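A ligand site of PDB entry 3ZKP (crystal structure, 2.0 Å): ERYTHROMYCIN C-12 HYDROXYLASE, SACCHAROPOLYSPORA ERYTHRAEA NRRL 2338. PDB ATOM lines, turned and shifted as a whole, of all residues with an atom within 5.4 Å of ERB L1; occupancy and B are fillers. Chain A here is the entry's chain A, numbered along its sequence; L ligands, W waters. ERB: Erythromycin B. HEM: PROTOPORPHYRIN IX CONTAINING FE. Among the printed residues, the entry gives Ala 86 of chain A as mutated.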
ATOM      1  N   PRO A  73     -17.939  -8.032 -24.195  1.00  0.00           N
ATOM      2  CA  PRO A  73     -18.077  -9.163 -25.098  1.00  0.00           C
ATOM      3  C   PRO A  73     -16.712  -9.622 -25.625  1.00  0.00           C
ATOM      4  O   PRO A  73     -16.593 -10.778 -26.031  1.00  0.00           O
ATOM      5  CB  PRO A  73     -18.900  -8.585 -26.253  1.00  0.00           C
ATOM      6  CG  PRO A  73     -18.536  -7.127 -26.266  1.00  0.00           C
ATOM      7  CD  PRO A  73     -18.416  -6.774 -24.809  1.00  0.00           C
ATOM      8  N   THR A  83     -12.925  -2.166 -25.737  1.00  0.00           N
ATOM      9  CA  THR A  83     -13.089  -0.848 -26.321  1.00  0.00           C
ATOM     10  C   THR A  83     -13.023   0.230 -25.236  1.00  0.00           C
ATOM     11  O   THR A  83     -13.893   0.280 -24.344  1.00  0.00           O
ATOM     12  CB  THR A  83     -14.401  -0.733 -27.113  1.00  0.00           C
ATOM     13  OG1 THR A  83     -14.418  -1.723 -28.155  1.00  0.00           O
ATOM     14  CG2 THR A  83     -14.563   0.623 -27.735  1.00  0.00           C
ATOM     15  N   ALA A  86     -16.113   2.496 -23.601  1.00  0.00           N
ATOM     16  CA  ALA A  86     -17.411   1.880 -23.862  1.00  0.00           C
ATOM     17  C   ALA A  86     -18.130   1.524 -22.547  1.00  0.00           C
ATOM     18  O   ALA A  86     -18.072   0.375 -22.080  1.00  0.00           O
ATOM     19  CB  ALA A  86     -17.244   0.650 -24.781  1.00  0.00           C
ATOM     20  N   ILE A  87     -18.797   2.506 -21.950  1.00  0.00           N
ATOM     21  CA  ILE A  87     -19.381   2.369 -20.600  1.00  0.00           C
ATOM     22  C   ILE A  87     -20.222   1.091 -20.427  1.00  0.00           C
ATOM     23  O   ILE A  87     -20.162   0.431 -19.378  1.00  0.00           O
ATOM     24  CB  ILE A  87     -20.194   3.649 -20.171  1.00  0.00           C
ATOM     25  CG1 ILE A  87     -20.684   3.522 -18.726  1.00  0.00           C
ATOM     26  CG2 ILE A  87     -21.344   3.962 -21.198  1.00  0.00           C
ATOM     27  CD1 ILE A  87     -21.533   4.738 -18.230  1.00  0.00           C
ATOM     28  N   HIS A  88     -20.965   0.766 -21.483  1.00  0.00           N
ATOM     29  CA  HIS A  88     -21.869  -0.390 -21.516  1.00  0.00           C
ATOM     30  C   HIS A  88     -21.141  -1.735 -21.557  1.00  0.00           C
ATOM     31  O   HIS A  88     -21.772  -2.800 -21.398  1.00  0.00           O
ATOM     32  CB  HIS A  88     -22.796  -0.273 -22.740  1.00  0.00           C
ATOM     33  CG  HIS A  88     -22.050  -0.159 -24.040  1.00  0.00           C
ATOM     34  ND1 HIS A  88     -21.228   0.910 -24.334  1.00  0.00           N
ATOM     35  CD2 HIS A  88     -21.994  -0.994 -25.108  1.00  0.00           C
ATOM     36  CE1 HIS A  88     -20.697   0.734 -25.534  1.00  0.00           C
ATOM     37  NE2 HIS A  88     -21.143  -0.407 -26.022  1.00  0.00           N
ATOM     38  N   GLU A  89     -19.814  -1.692 -21.767  1.00  0.00           N
ATOM     39  CA  GLU A  89     -18.973  -2.894 -21.835  1.00  0.00           C
ATOM     40  C   GLU A  89     -17.897  -2.956 -20.730  1.00  0.00           C
ATOM     41  O   GLU A  89     -17.047  -3.869 -20.714  1.00  0.00           O
ATOM     42  CB  GLU A  89     -18.333  -3.043 -23.218  1.00  0.00           C
ATOM     43  CG  GLU A  89     -19.362  -3.312 -24.330  1.00  0.00           C
ATOM     44  CD  GLU A  89     -18.729  -3.488 -25.710  1.00  0.00           C
ATOM     45  OE1 GLU A  89     -17.479  -3.440 -25.819  1.00  0.00           O
ATOM     46  OE2 GLU A  89     -19.497  -3.677 -26.691  1.00  0.00           O
ATOM     47  N   LEU A 169     -26.364   0.261 -38.486  1.00  0.00           N
ATOM     48  CA  LEU A 169     -25.911  -0.515 -37.354  1.00  0.00           C
ATOM     49  C   LEU A 169     -26.960  -1.537 -37.053  1.00  0.00           C
ATOM     50  O   LEU A 169     -26.665  -2.717 -36.955  1.00  0.00           O
ATOM     51  CB  LEU A 169     -25.636   0.379 -36.122  1.00  0.00           C
ATOM     52  CG  LEU A 169     -25.220  -0.313 -34.815  1.00  0.00           C
ATOM     53  CD1 LEU A 169     -23.902  -1.074 -34.989  1.00  0.00           C
ATOM     54  CD2 LEU A 169     -25.110   0.688 -33.668  1.00  0.00           C
ATOM     55  N   VAL A 170     -28.207  -1.079 -36.970  1.00  0.00           N
ATOM     56  CA  VAL A 170     -29.333  -1.971 -36.683  1.00  0.00           C
ATOM     57  C   VAL A 170     -29.542  -3.067 -37.746  1.00  0.00           C
ATOM     58  O   VAL A 170     -29.990  -4.162 -37.389  1.00  0.00           O
ATOM     59  CB  VAL A 170     -30.641  -1.159 -36.383  1.00  0.00           C
ATOM     60  CG1 VAL A 170     -31.867  -2.058 -36.347  1.00  0.00           C
ATOM     61  CG2 VAL A 170     -30.506  -0.450 -35.048  1.00  0.00           C
ATOM     62  N   ILE A 172     -26.994  -4.361 -39.719  1.00  0.00           N
ATOM     63  CA  ILE A 172     -25.722  -4.994 -40.024  1.00  0.00           C
ATOM     64  C   ILE A 172     -25.904  -6.506 -40.210  1.00  0.00           C
ATOM     65  O   ILE A 172     -26.696  -7.135 -39.495  1.00  0.00           O
ATOM     66  CB  ILE A 172     -24.638  -4.657 -38.957  1.00  0.00           C
ATOM     67  CG1 ILE A 172     -23.246  -4.907 -39.516  1.00  0.00           C
ATOM     68  CG2 ILE A 172     -24.881  -5.400 -37.643  1.00  0.00           C
ATOM     69  CD1 ILE A 172     -22.160  -4.381 -38.636  1.00  0.00           C
ATOM     70  N   MET A 174     -25.507 -10.085 -39.563  1.00  0.00           N
ATOM     71  CA  MET A 174     -25.135 -10.681 -38.291  1.00  0.00           C
ATOM     72  C   MET A 174     -25.771 -12.040 -37.979  1.00  0.00           C
ATOM     73  O   MET A 174     -26.967 -12.215 -38.105  1.00  0.00           O
ATOM     74  CB  MET A 174     -25.605  -9.762 -37.159  1.00  0.00           C
ATOM     75  CG  MET A 174     -25.520 -10.338 -35.761  1.00  0.00           C
ATOM     76  SD  MET A 174     -26.160  -9.163 -34.547  1.00  0.00           S
ATOM     77  CE  MET A 174     -27.905  -9.552 -34.445  1.00  0.00           C
ATOM     78  N   PRO A 177     -22.962 -13.931 -32.779  1.00  0.00           N
ATOM     79  CA  PRO A 177     -22.552 -12.665 -32.145  1.00  0.00           C
ATOM     80  C   PRO A 177     -21.146 -12.668 -31.543  1.00  0.00           C
ATOM     81  O   PRO A 177     -20.669 -11.615 -31.097  1.00  0.00           O
ATOM     82  CB  PRO A 177     -23.604 -12.486 -31.037  1.00  0.00           C
ATOM     83  CG  PRO A 177     -24.024 -13.861 -30.678  1.00  0.00           C
ATOM     84  CD  PRO A 177     -23.949 -14.671 -31.962  1.00  0.00           C
ATOM     85  N   LEU A 182     -17.794  -9.959 -37.170  1.00  0.00           N
ATOM     86  CA  LEU A 182     -18.914  -9.058 -36.815  1.00  0.00           C
ATOM     87  C   LEU A 182     -18.400  -7.823 -36.036  1.00  0.00           C
ATOM     88  O   LEU A 182     -18.813  -6.701 -36.317  1.00  0.00           O
ATOM     89  CB  LEU A 182     -20.023  -9.769 -36.023  1.00  0.00           C
ATOM     90  CG  LEU A 182     -21.124  -8.882 -35.406  1.00  0.00           C
ATOM     91  CD1 LEU A 182     -22.020  -8.212 -36.455  1.00  0.00           C
ATOM     92  CD2 LEU A 182     -21.969  -9.643 -34.399  1.00  0.00           C
ATOM     93  N   ILE A 186     -18.961  -4.040 -37.206  1.00  0.00           N
ATOM     94  CA  ILE A 186     -19.538  -2.976 -36.363  1.00  0.00           C
ATOM     95  C   ILE A 186     -18.611  -1.760 -36.338  1.00  0.00           C
ATOM     96  O   ILE A 186     -19.055  -0.645 -36.623  1.00  0.00           O
ATOM     97  CB  ILE A 186     -19.848  -3.462 -34.920  1.00  0.00           C
ATOM     98  CG1 ILE A 186     -20.921  -4.550 -34.950  1.00  0.00           C
ATOM     99  CG2 ILE A 186     -20.290  -2.278 -34.015  1.00  0.00           C
ATOM    100  CD1 ILE A 186     -21.061  -5.328 -33.634  1.00  0.00           C
ATOM    101  N   LEU A 190     -19.521   2.041 -37.741  1.00  0.00           N
ATOM    102  CA  LEU A 190     -19.528   3.157 -36.797  1.00  0.00           C
ATOM    103  C   LEU A 190     -18.332   4.094 -36.937  1.00  0.00           C
ATOM    104  O   LEU A 190     -18.273   5.122 -36.244  1.00  0.00           O
ATOM    105  CB  LEU A 190     -19.622   2.643 -35.355  1.00  0.00           C
ATOM    106  CG  LEU A 190     -20.943   2.023 -34.911  1.00  0.00           C
ATOM    107  CD1 LEU A 190     -20.785   1.592 -33.444  1.00  0.00           C
ATOM    108  CD2 LEU A 190     -22.139   2.981 -35.071  1.00  0.00           C
ATOM    109  N   THR A 236     -19.890   8.292 -28.526  1.00  0.00           N
ATOM    110  CA  THR A 236     -20.587   7.416 -29.479  1.00  0.00           C
ATOM    111  C   THR A 236     -21.668   6.606 -28.758  1.00  0.00           C
ATOM    112  O   THR A 236     -22.808   6.580 -29.210  1.00  0.00           O
ATOM    113  CB  THR A 236     -19.586   6.514 -30.243  1.00  0.00           C
ATOM    114  OG1 THR A 236     -18.661   7.351 -30.963  1.00  0.00           O
ATOM    115  CG2 THR A 236     -20.312   5.553 -31.226  1.00  0.00           C
ATOM    116  N   ALA A 237     -21.312   5.990 -27.618  1.00  0.00           N
ATOM    117  CA  ALA A 237     -22.291   5.254 -26.801  1.00  0.00           C
ATOM    118  C   ALA A 237     -23.438   6.154 -26.348  1.00  0.00           C
ATOM    119  O   ALA A 237     -24.592   5.731 -26.425  1.00  0.00           O
ATOM    120  CB  ALA A 237     -21.603   4.565 -25.586  1.00  0.00           C
ATOM    121  N   LEU A 238     -23.150   7.364 -25.877  1.00  0.00           N
ATOM    122  CA  LEU A 238     -24.188   8.299 -25.444  1.00  0.00           C
ATOM    123  C   LEU A 238     -25.149   8.696 -26.568  1.00  0.00           C
ATOM    124  O   LEU A 238     -26.357   8.784 -26.352  1.00  0.00           O
ATOM    125  CB  LEU A 238     -23.590   9.540 -24.776  1.00  0.00           C
ATOM    126  CG  LEU A 238     -22.910   9.317 -23.407  1.00  0.00           C
ATOM    127  CD1 LEU A 238     -21.942  10.461 -23.116  1.00  0.00           C
ATOM    128  CD2 LEU A 238     -23.951   9.146 -22.298  1.00  0.00           C
ATOM    129  N   LEU A 240     -25.862   7.049 -29.526  1.00  0.00           N
ATOM    130  CA  LEU A 240     -26.677   5.915 -29.939  1.00  0.00           C
ATOM    131  C   LEU A 240     -27.720   5.554 -28.868  1.00  0.00           C
ATOM    132  O   LEU A 240     -28.896   5.363 -29.185  1.00  0.00           O
ATOM    133  CB  LEU A 240     -25.772   4.726 -30.277  1.00  0.00           C
ATOM    134  CG  LEU A 240     -24.806   4.892 -31.458  1.00  0.00           C
ATOM    135  CD1 LEU A 240     -23.730   3.828 -31.350  1.00  0.00           C
ATOM    136  CD2 LEU A 240     -25.543   4.782 -32.839  1.00  0.00           C
ATOM    137  N   ALA A 241     -27.282   5.493 -27.608  1.00  0.00           N
ATOM    138  CA  ALA A 241     -28.165   5.193 -26.482  1.00  0.00           C
ATOM    139  C   ALA A 241     -29.350   6.132 -26.422  1.00  0.00           C
ATOM    140  O   ALA A 241     -30.442   5.736 -26.000  1.00  0.00           O
ATOM    141  CB  ALA A 241     -27.389   5.244 -25.187  1.00  0.00           C
ATOM    142  N   ILE A 244     -32.190   5.680 -30.528  1.00  0.00           N
ATOM    143  CA  ILE A 244     -32.786   4.492 -31.175  1.00  0.00           C
ATOM    144  C   ILE A 244     -33.974   3.892 -30.373  1.00  0.00           C
ATOM    145  O   ILE A 244     -35.063   3.730 -30.907  1.00  0.00           O
ATOM    146  CB  ILE A 244     -31.708   3.384 -31.500  1.00  0.00           C
ATOM    147  CG1 ILE A 244     -30.500   4.004 -32.230  1.00  0.00           C
ATOM    148  CG2 ILE A 244     -32.394   2.262 -32.285  1.00  0.00           C
ATOM    149  CD1 ILE A 244     -29.251   3.034 -32.501  1.00  0.00           C
ATOM    150  N   THR A 245     -33.744   3.592 -29.103  1.00  0.00           N
ATOM    151  CA  THR A 245     -34.778   2.985 -28.266  1.00  0.00           C
ATOM    152  C   THR A 245     -35.972   3.899 -27.967  1.00  0.00           C
ATOM    153  O   THR A 245     -37.125   3.439 -27.873  1.00  0.00           O
ATOM    154  CB  THR A 245     -34.168   2.553 -26.944  1.00  0.00           C
ATOM    155  OG1 THR A 245     -33.287   3.593 -26.494  1.00  0.00           O
ATOM    156  CG2 THR A 245     -33.391   1.252 -27.108  1.00  0.00           C
ATOM    157  N   PRO A 287     -38.146  -2.145 -26.236  1.00  0.00           N
ATOM    158  CA  PRO A 287     -37.367  -1.820 -27.443  1.00  0.00           C
ATOM    159  C   PRO A 287     -36.122  -2.709 -27.668  1.00  0.00           C
ATOM    160  O   PRO A 287     -35.844  -3.112 -28.807  1.00  0.00           O
ATOM    161  CB  PRO A 287     -36.973  -0.338 -27.209  1.00  0.00           C
ATOM    162  CG  PRO A 287     -38.166   0.218 -26.384  1.00  0.00           C
ATOM    163  CD  PRO A 287     -38.441  -0.947 -25.423  1.00  0.00           C
ATOM    164  N   PHE A 288     -35.411  -3.015 -26.588  1.00  0.00           N
ATOM    165  CA  PHE A 288     -34.198  -3.811 -26.618  1.00  0.00           C
ATOM    166  C   PHE A 288     -34.562  -5.115 -25.892  1.00  0.00           C
ATOM    167  O   PHE A 288     -34.556  -5.155 -24.672  1.00  0.00           O
ATOM    168  CB  PHE A 288     -33.080  -3.053 -25.876  1.00  0.00           C
ATOM    169  CG  PHE A 288     -31.672  -3.593 -26.084  1.00  0.00           C
ATOM    170  CD1 PHE A 288     -31.190  -3.856 -27.369  1.00  0.00           C
ATOM    171  CD2 PHE A 288     -30.800  -3.720 -25.000  1.00  0.00           C
ATOM    172  CE1 PHE A 288     -29.878  -4.294 -27.569  1.00  0.00           C
ATOM    173  CE2 PHE A 288     -29.485  -4.165 -25.188  1.00  0.00           C
ATOM    174  CZ  PHE A 288     -29.023  -4.435 -26.455  1.00  0.00           C
ATOM    175  N   GLN A 290     -33.237  -8.158 -25.717  1.00  0.00           N
ATOM    176  CA  GLN A 290     -32.166  -9.032 -25.242  1.00  0.00           C
ATOM    177  C   GLN A 290     -30.856  -8.254 -25.069  1.00  0.00           C
ATOM    178  O   GLN A 290     -30.633  -7.227 -25.717  1.00  0.00           O
ATOM    179  CB  GLN A 290     -31.963 -10.199 -26.228  1.00  0.00           C
ATOM    180  CG  GLN A 290     -31.479  -9.702 -27.564  1.00  0.00           C
ATOM    181  CD  GLN A 290     -31.307 -10.770 -28.645  1.00  0.00           C
ATOM    182  OE1 GLN A 290     -31.534 -11.966 -28.441  1.00  0.00           O
ATOM    183  NE2 GLN A 290     -30.905 -10.304 -29.834  1.00  0.00           N
ATOM    184  N   GLN A 292     -26.408  -9.017 -23.917  1.00  0.00           N
ATOM    185  CA  GLN A 292     -25.401 -10.052 -23.722  1.00  0.00           C
ATOM    186  C   GLN A 292     -24.463  -9.774 -22.555  1.00  0.00           C
ATOM    187  O   GLN A 292     -24.219  -8.616 -22.184  1.00  0.00           O
ATOM    188  CB  GLN A 292     -24.605 -10.333 -25.006  1.00  0.00           C
ATOM    189  CG  GLN A 292     -25.444 -10.917 -26.156  1.00  0.00           C
ATOM    190  CD  GLN A 292     -26.177  -9.841 -26.932  1.00  0.00           C
ATOM    191  OE1 GLN A 292     -25.561  -8.897 -27.421  1.00  0.00           O
ATOM    192  NE2 GLN A 292     -27.497  -9.947 -27.018  1.00  0.00           N
ATOM    193  N   ILE A 392     -32.319  -7.268 -33.577  1.00  0.00           N
ATOM    194  CA  ILE A 392     -31.733  -6.368 -32.563  1.00  0.00           C
ATOM    195  C   ILE A 392     -32.754  -5.597 -31.708  1.00  0.00           C
ATOM    196  O   ILE A 392     -32.698  -5.663 -30.475  1.00  0.00           O
ATOM    197  CB  ILE A 392     -30.645  -5.405 -33.166  1.00  0.00           C
ATOM    198  CG1 ILE A 392     -29.513  -6.244 -33.807  1.00  0.00           C
ATOM    199  CG2 ILE A 392     -30.065  -4.463 -32.069  1.00  0.00           C
ATOM    200  CD1 ILE A 392     -28.416  -5.443 -34.504  1.00  0.00           C
ATOM    201  N   VAL A 393     -33.671  -4.888 -32.346  1.00  0.00           N
ATOM    202  CA  VAL A 393     -34.730  -4.163 -31.581  1.00  0.00           C
ATOM    203  C   VAL A 393     -36.120  -4.740 -31.853  1.00  0.00           C
ATOM    204  O   VAL A 393     -36.336  -5.400 -32.871  1.00  0.00           O
ATOM    205  CB  VAL A 393     -34.717  -2.657 -31.893  1.00  0.00           C
ATOM    206  CG1 VAL A 393     -33.420  -2.038 -31.438  1.00  0.00           C
ATOM    207  CG2 VAL A 393     -34.922  -2.397 -33.409  1.00  0.00           C
HETATM  208  C1  ERB L   1     -25.092   1.242 -27.219  1.00  0.00           C
HETATM  209  N1  ERB L   1     -26.133  -8.109 -30.207  1.00  0.00           N
HETATM  210  O1  ERB L   1     -25.875   1.904 -27.879  1.00  0.00           O
HETATM  211  C2  ERB L   1     -23.801   0.634 -27.741  1.00  0.00           C
HETATM  212  O2  ERB L   1     -25.337   0.983 -25.825  1.00  0.00           O
HETATM  213  C3  ERB L   1     -24.044  -0.422 -28.848  1.00  0.00           C
HETATM  214  O3  ERB L   1     -22.820  -1.167 -28.978  1.00  0.00           O
HETATM  215  C4  ERB L   1     -25.219  -1.353 -28.511  1.00  0.00           C
HETATM  216  O4  ERB L   1     -22.336  -2.960 -30.386  1.00  0.00           O
HETATM  217  C5  ERB L   1     -25.926  -1.892 -29.781  1.00  0.00           C
HETATM  218  O5  ERB L   1     -19.756  -1.028 -28.674  1.00  0.00           O
HETATM  219  C6  ERB L   1     -27.142  -1.071 -30.229  1.00  0.00           C
HETATM  220  O6  ERB L   1     -18.936  -3.650 -29.248  1.00  0.00           O
HETATM  221  C7  ERB L   1     -28.317  -1.375 -29.282  1.00  0.00           C
HETATM  222  O7  ERB L   1     -26.395  -3.231 -29.580  1.00  0.00           O
HETATM  223  C8  ERB L   1     -29.355  -0.270 -29.012  1.00  0.00           C
HETATM  224  O8  ERB L   1     -26.438  -5.831 -28.403  1.00  0.00           O
HETATM  225  C9  ERB L   1     -30.155  -0.566 -27.740  1.00  0.00           C
HETATM  226  O9  ERB L   1     -25.580  -4.142 -31.573  1.00  0.00           O
HETATM  227  C10 ERB L   1     -29.533  -0.460 -26.346  1.00  0.00           C
HETATM  228  O10 ERB L   1     -26.812   0.324 -30.226  1.00  0.00           O
HETATM  229  C11 ERB L   1     -28.442   0.617 -26.311  1.00  0.00           C
HETATM  230  O11 ERB L   1     -31.315  -0.921 -27.820  1.00  0.00           O
HETATM  231  C12 ERB L   1     -27.585   0.615 -25.036  1.00  0.00           C
HETATM  232  O12 ERB L   1     -29.064   1.886 -26.518  1.00  0.00           O
HETATM  233  C13 ERB L   1     -26.418   1.599 -25.158  1.00  0.00           C
HETATM  234  C14 ERB L   1     -22.410  -1.520 -30.310  1.00  0.00           C
HETATM  235  C15 ERB L   1     -21.069  -0.862 -30.697  1.00  0.00           C
HETATM  236  C16 ERB L   1     -19.832  -1.503 -30.021  1.00  0.00           C
HETATM  237  C17 ERB L   1     -19.966  -3.032 -30.021  1.00  0.00           C
HETATM  238  C18 ERB L   1     -21.345  -3.520 -29.536  1.00  0.00           C
HETATM  239  C19 ERB L   1     -18.571  -1.029 -30.789  1.00  0.00           C
HETATM  240  C20 ERB L   1     -18.536  -0.545 -28.073  1.00  0.00           C
HETATM  241  C21 ERB L   1     -21.483  -5.037 -29.570  1.00  0.00           C
HETATM  242  C22 ERB L   1     -25.628  -4.303 -30.155  1.00  0.00           C
HETATM  243  C23 ERB L   1     -26.276  -5.644 -29.838  1.00  0.00           C
HETATM  244  C24 ERB L   1     -25.495  -6.791 -30.501  1.00  0.00           C
HETATM  245  C25 ERB L   1     -25.309  -6.502 -32.012  1.00  0.00           C
HETATM  246  C26 ERB L   1     -24.739  -5.097 -32.229  1.00  0.00           C
HETATM  247  C27 ERB L   1     -24.693  -4.732 -33.724  1.00  0.00           C
HETATM  248  C28 ERB L   1     -27.465  -8.343 -30.837  1.00  0.00           C
HETATM  249  C29 ERB L   1     -25.233  -9.206 -30.592  1.00  0.00           C
HETATM  250  C30 ERB L   1     -22.805   1.749 -28.108  1.00  0.00           C
HETATM  251  C31 ERB L   1     -24.785  -2.455 -27.531  1.00  0.00           C
HETATM  252  C32 ERB L   1     -27.512  -1.437 -31.682  1.00  0.00           C
HETATM  253  C33 ERB L   1     -30.277  -0.087 -30.226  1.00  0.00           C
HETATM  254  C34 ERB L   1     -30.580  -0.232 -25.246  1.00  0.00           C
HETATM  255  C35 ERB L   1     -27.147  -0.811 -24.656  1.00  0.00           C
HETATM  256  C36 ERB L   1     -25.832   1.961 -23.793  1.00  0.00           C
HETATM  257  C37 ERB L   1     -24.770   3.027 -23.956  1.00  0.00           C
HETATM  258  CHA HEM L   2     -28.183   1.639 -20.686  1.00  0.00           C
HETATM  259  CHB HEM L   2     -32.650   0.852 -22.433  1.00  0.00           C
HETATM  260  CHC HEM L   2     -33.193   5.533 -23.531  1.00  0.00           C
HETATM  261  CHD HEM L   2     -28.578   6.373 -22.089  1.00  0.00           C
HETATM  262  C1A HEM L   2     -29.356   0.999 -21.046  1.00  0.00           C
HETATM  263  C2A HEM L   2     -29.699  -0.394 -20.836  1.00  0.00           C
HETATM  264  C3A HEM L   2     -30.937  -0.604 -21.313  1.00  0.00           C
HETATM  265  C4A HEM L   2     -31.424   0.645 -21.844  1.00  0.00           C
HETATM  266  CMA HEM L   2     -31.724  -1.958 -21.313  1.00  0.00           C
HETATM  267  CAA HEM L   2     -28.782  -1.437 -20.161  1.00  0.00           C
HETATM  268  CBA HEM L   2     -28.006  -2.294 -21.152  1.00  0.00           C
HETATM  269  CGA HEM L   2     -27.172  -3.359 -20.424  1.00  0.00           C
HETATM  270  O1A HEM L   2     -27.424  -3.686 -19.225  1.00  0.00           O
HETATM  271  O2A HEM L   2     -26.245  -3.915 -21.065  1.00  0.00           O
HETATM  272  C1B HEM L   2     -33.216   2.030 -22.882  1.00  0.00           C
HETATM  273  C2B HEM L   2     -34.548   2.198 -23.429  1.00  0.00           C
HETATM  274  C3B HEM L   2     -34.714   3.494 -23.733  1.00  0.00           C
HETATM  275  C4B HEM L   2     -33.480   4.189 -23.393  1.00  0.00           C
HETATM  276  CMB HEM L   2     -35.536   1.017 -23.593  1.00  0.00           C
HETATM  277  CAB HEM L   2     -35.940   4.212 -24.369  1.00  0.00           C
HETATM  278  CBB HEM L   2     -37.218   3.997 -24.019  1.00  0.00           C
HETATM  279  C1C HEM L   2     -32.004   6.170 -23.219  1.00  0.00           C
HETATM  280  C2C HEM L   2     -31.746   7.585 -23.385  1.00  0.00           C
HETATM  281  C3C HEM L   2     -30.472   7.818 -22.989  1.00  0.00           C
HETATM  282  C4C HEM L   2     -29.882   6.565 -22.564  1.00  0.00           C
HETATM  283  CMC HEM L   2     -32.780   8.613 -23.902  1.00  0.00           C
HETATM  284  CAC HEM L   2     -29.762   9.185 -22.993  1.00  0.00           C
HETATM  285  CBC HEM L   2     -28.533   9.264 -23.522  1.00  0.00           C
HETATM  286  C1D HEM L   2     -28.034   5.190 -21.612  1.00  0.00           C
HETATM  287  C2D HEM L   2     -26.658   5.017 -21.180  1.00  0.00           C
HETATM  288  C3D HEM L   2     -26.553   3.560 -20.765  1.00  0.00           C
HETATM  289  C4D HEM L   2     -27.859   2.972 -20.950  1.00  0.00           C
HETATM  290  CMD HEM L   2     -25.523   6.067 -21.206  1.00  0.00           C
HETATM  291  CAD HEM L   2     -25.315   2.832 -20.238  1.00  0.00           C
HETATM  292  CBD HEM L   2     -25.441   2.772 -18.717  1.00  0.00           C
HETATM  293  CGD HEM L   2     -24.279   2.011 -18.144  1.00  0.00           C
HETATM  294  O1D HEM L   2     -23.740   1.137 -18.862  1.00  0.00           O
HETATM  295  O2D HEM L   2     -23.917   2.277 -16.963  1.00  0.00           O
HETATM  296  NA  HEM L   2     -30.448   1.610 -21.664  1.00  0.00           N
HETATM  297  NB  HEM L   2     -32.592   3.269 -22.908  1.00  0.00           N
HETATM  298  NC  HEM L   2     -30.835   5.580 -22.737  1.00  0.00           N
HETATM  299  ND  HEM L   2     -28.697   3.965 -21.451  1.00  0.00           N
HETATM  300 FE   HEM L   2     -30.744   3.613 -22.019  1.00  0.00          FE
HETATM  301  O   HOH W   1     -30.245   3.288 -24.689  1.00  0.00           O
HETATM  302  O   HOH W   2     -28.819  -7.354 -27.679  1.00  0.00           O
HETATM  303  O   HOH W   3     -27.277 -11.719 -30.084  1.00  0.00           O
HETATM  304  O   HOH W   4     -30.517   3.362 -28.360  1.00  0.00           O
HETATM  305  O   HOH W   5     -30.615  -7.450 -29.712  1.00  0.00           O
HETATM  306  O   HOH W   6     -24.036  -6.067 -27.203  1.00  0.00           O
HETATM  307  O   HOH W   7     -16.273  -3.722 -28.231  1.00  0.00           O
HETATM  308  O   HOH W   8     -17.922  -5.530 -30.855  1.00  0.00           O
HETATM  309  O   HOH W   9     -25.937  -6.474 -25.048  1.00  0.00           O
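O6 of ERB L1 sits at hydrogen-bond distance from OE2 of Glu 89, 2.6 Å away. The side-chain amide oxygen of Gln 292 sits close to an oxygen (O8) of ERB L1. NE2 of His 88 is in hydrogen-bond range of O5 of ERB L1.
Ala 86 touches ERB L1 (CB to C20, 3.7 Å). CD2 of Leu 169 touches C32 of ERB L1 (3.8 Å). CG2 of Ile 172 touches C27 of ERB L1, at 3.98 Å. Met 174 touches ERB L1 (SD to C25, 3.8 Å). Pro 177 touches ERB L1 (CB to C29, 3.7 Å). Ile 186 touches ERB L1 (CD1 to C27, 3.7 Å). Leu 190 touches ERB L1 (CD1 to C15, 3.7 Å). Ala 237 touches ERB L1 (O to C37, 3.7 Å). CB of Leu 240 touches O1 of ERB L1, 3.7 Å away. CA of Ala 241 touches O12 of ERB L1, 3.4 Å away. CG2 of Ile 244 touches C33 of ERB L1 (3.8 Å). Thr 245 touches ERB L1 (CG2 to O11, 3.1 Å). Phe 288 touches ERB L1. CD1 of Ile 392 touches C27 of ERB L1, 3.9 Å away. Val 393 touches ERB L1 (CG1 to C33, 3.9 Å). Within 4 Å of ERB L1: Ala 86, His 88, Glu 89, Leu 169, Ile 172, Met 174, Pro 177, Ile 186, Leu 190, Ala 237, Leu 240, Ala 241, Ile 244, Thr 245, Phe 288, Gln 292, Ile 392 and Val 393. The nearest printed residue that does not touch ERB L1 is Gln 290 (4.1 Å).
Water W1 lies within hydrogen-bond range of O12 of ERB L1 (2.6 Å) and O of Ala 241 (2.8 Å). Water W6 bridges an oxygen (O8) of ERB L1 (2.7 Å) and the side-chain amide oxygen (OE1) of Gln 292 (3.2 Å). Water W7 lies within hydrogen-bond range of OE1 of Glu 89 (2.7 Å), OG1 of Thr 83 (2.7 Å) and O6 of ERB L1 (2.9 Å). Water W2 lies within hydrogen-bond range of O of Gln 290, O8 of ERB L1 and NE2 of Gln 292. Water W9 bridges N of Gln 292 (2.8 Å) and O8 of ERB L1 (3.5 Å). Water W5 lies within hydrogen-bond range of the backbone carbonyl oxygen (O) of Ile 392 and the side-chain amide nitrogen (NE2) of Gln 290.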
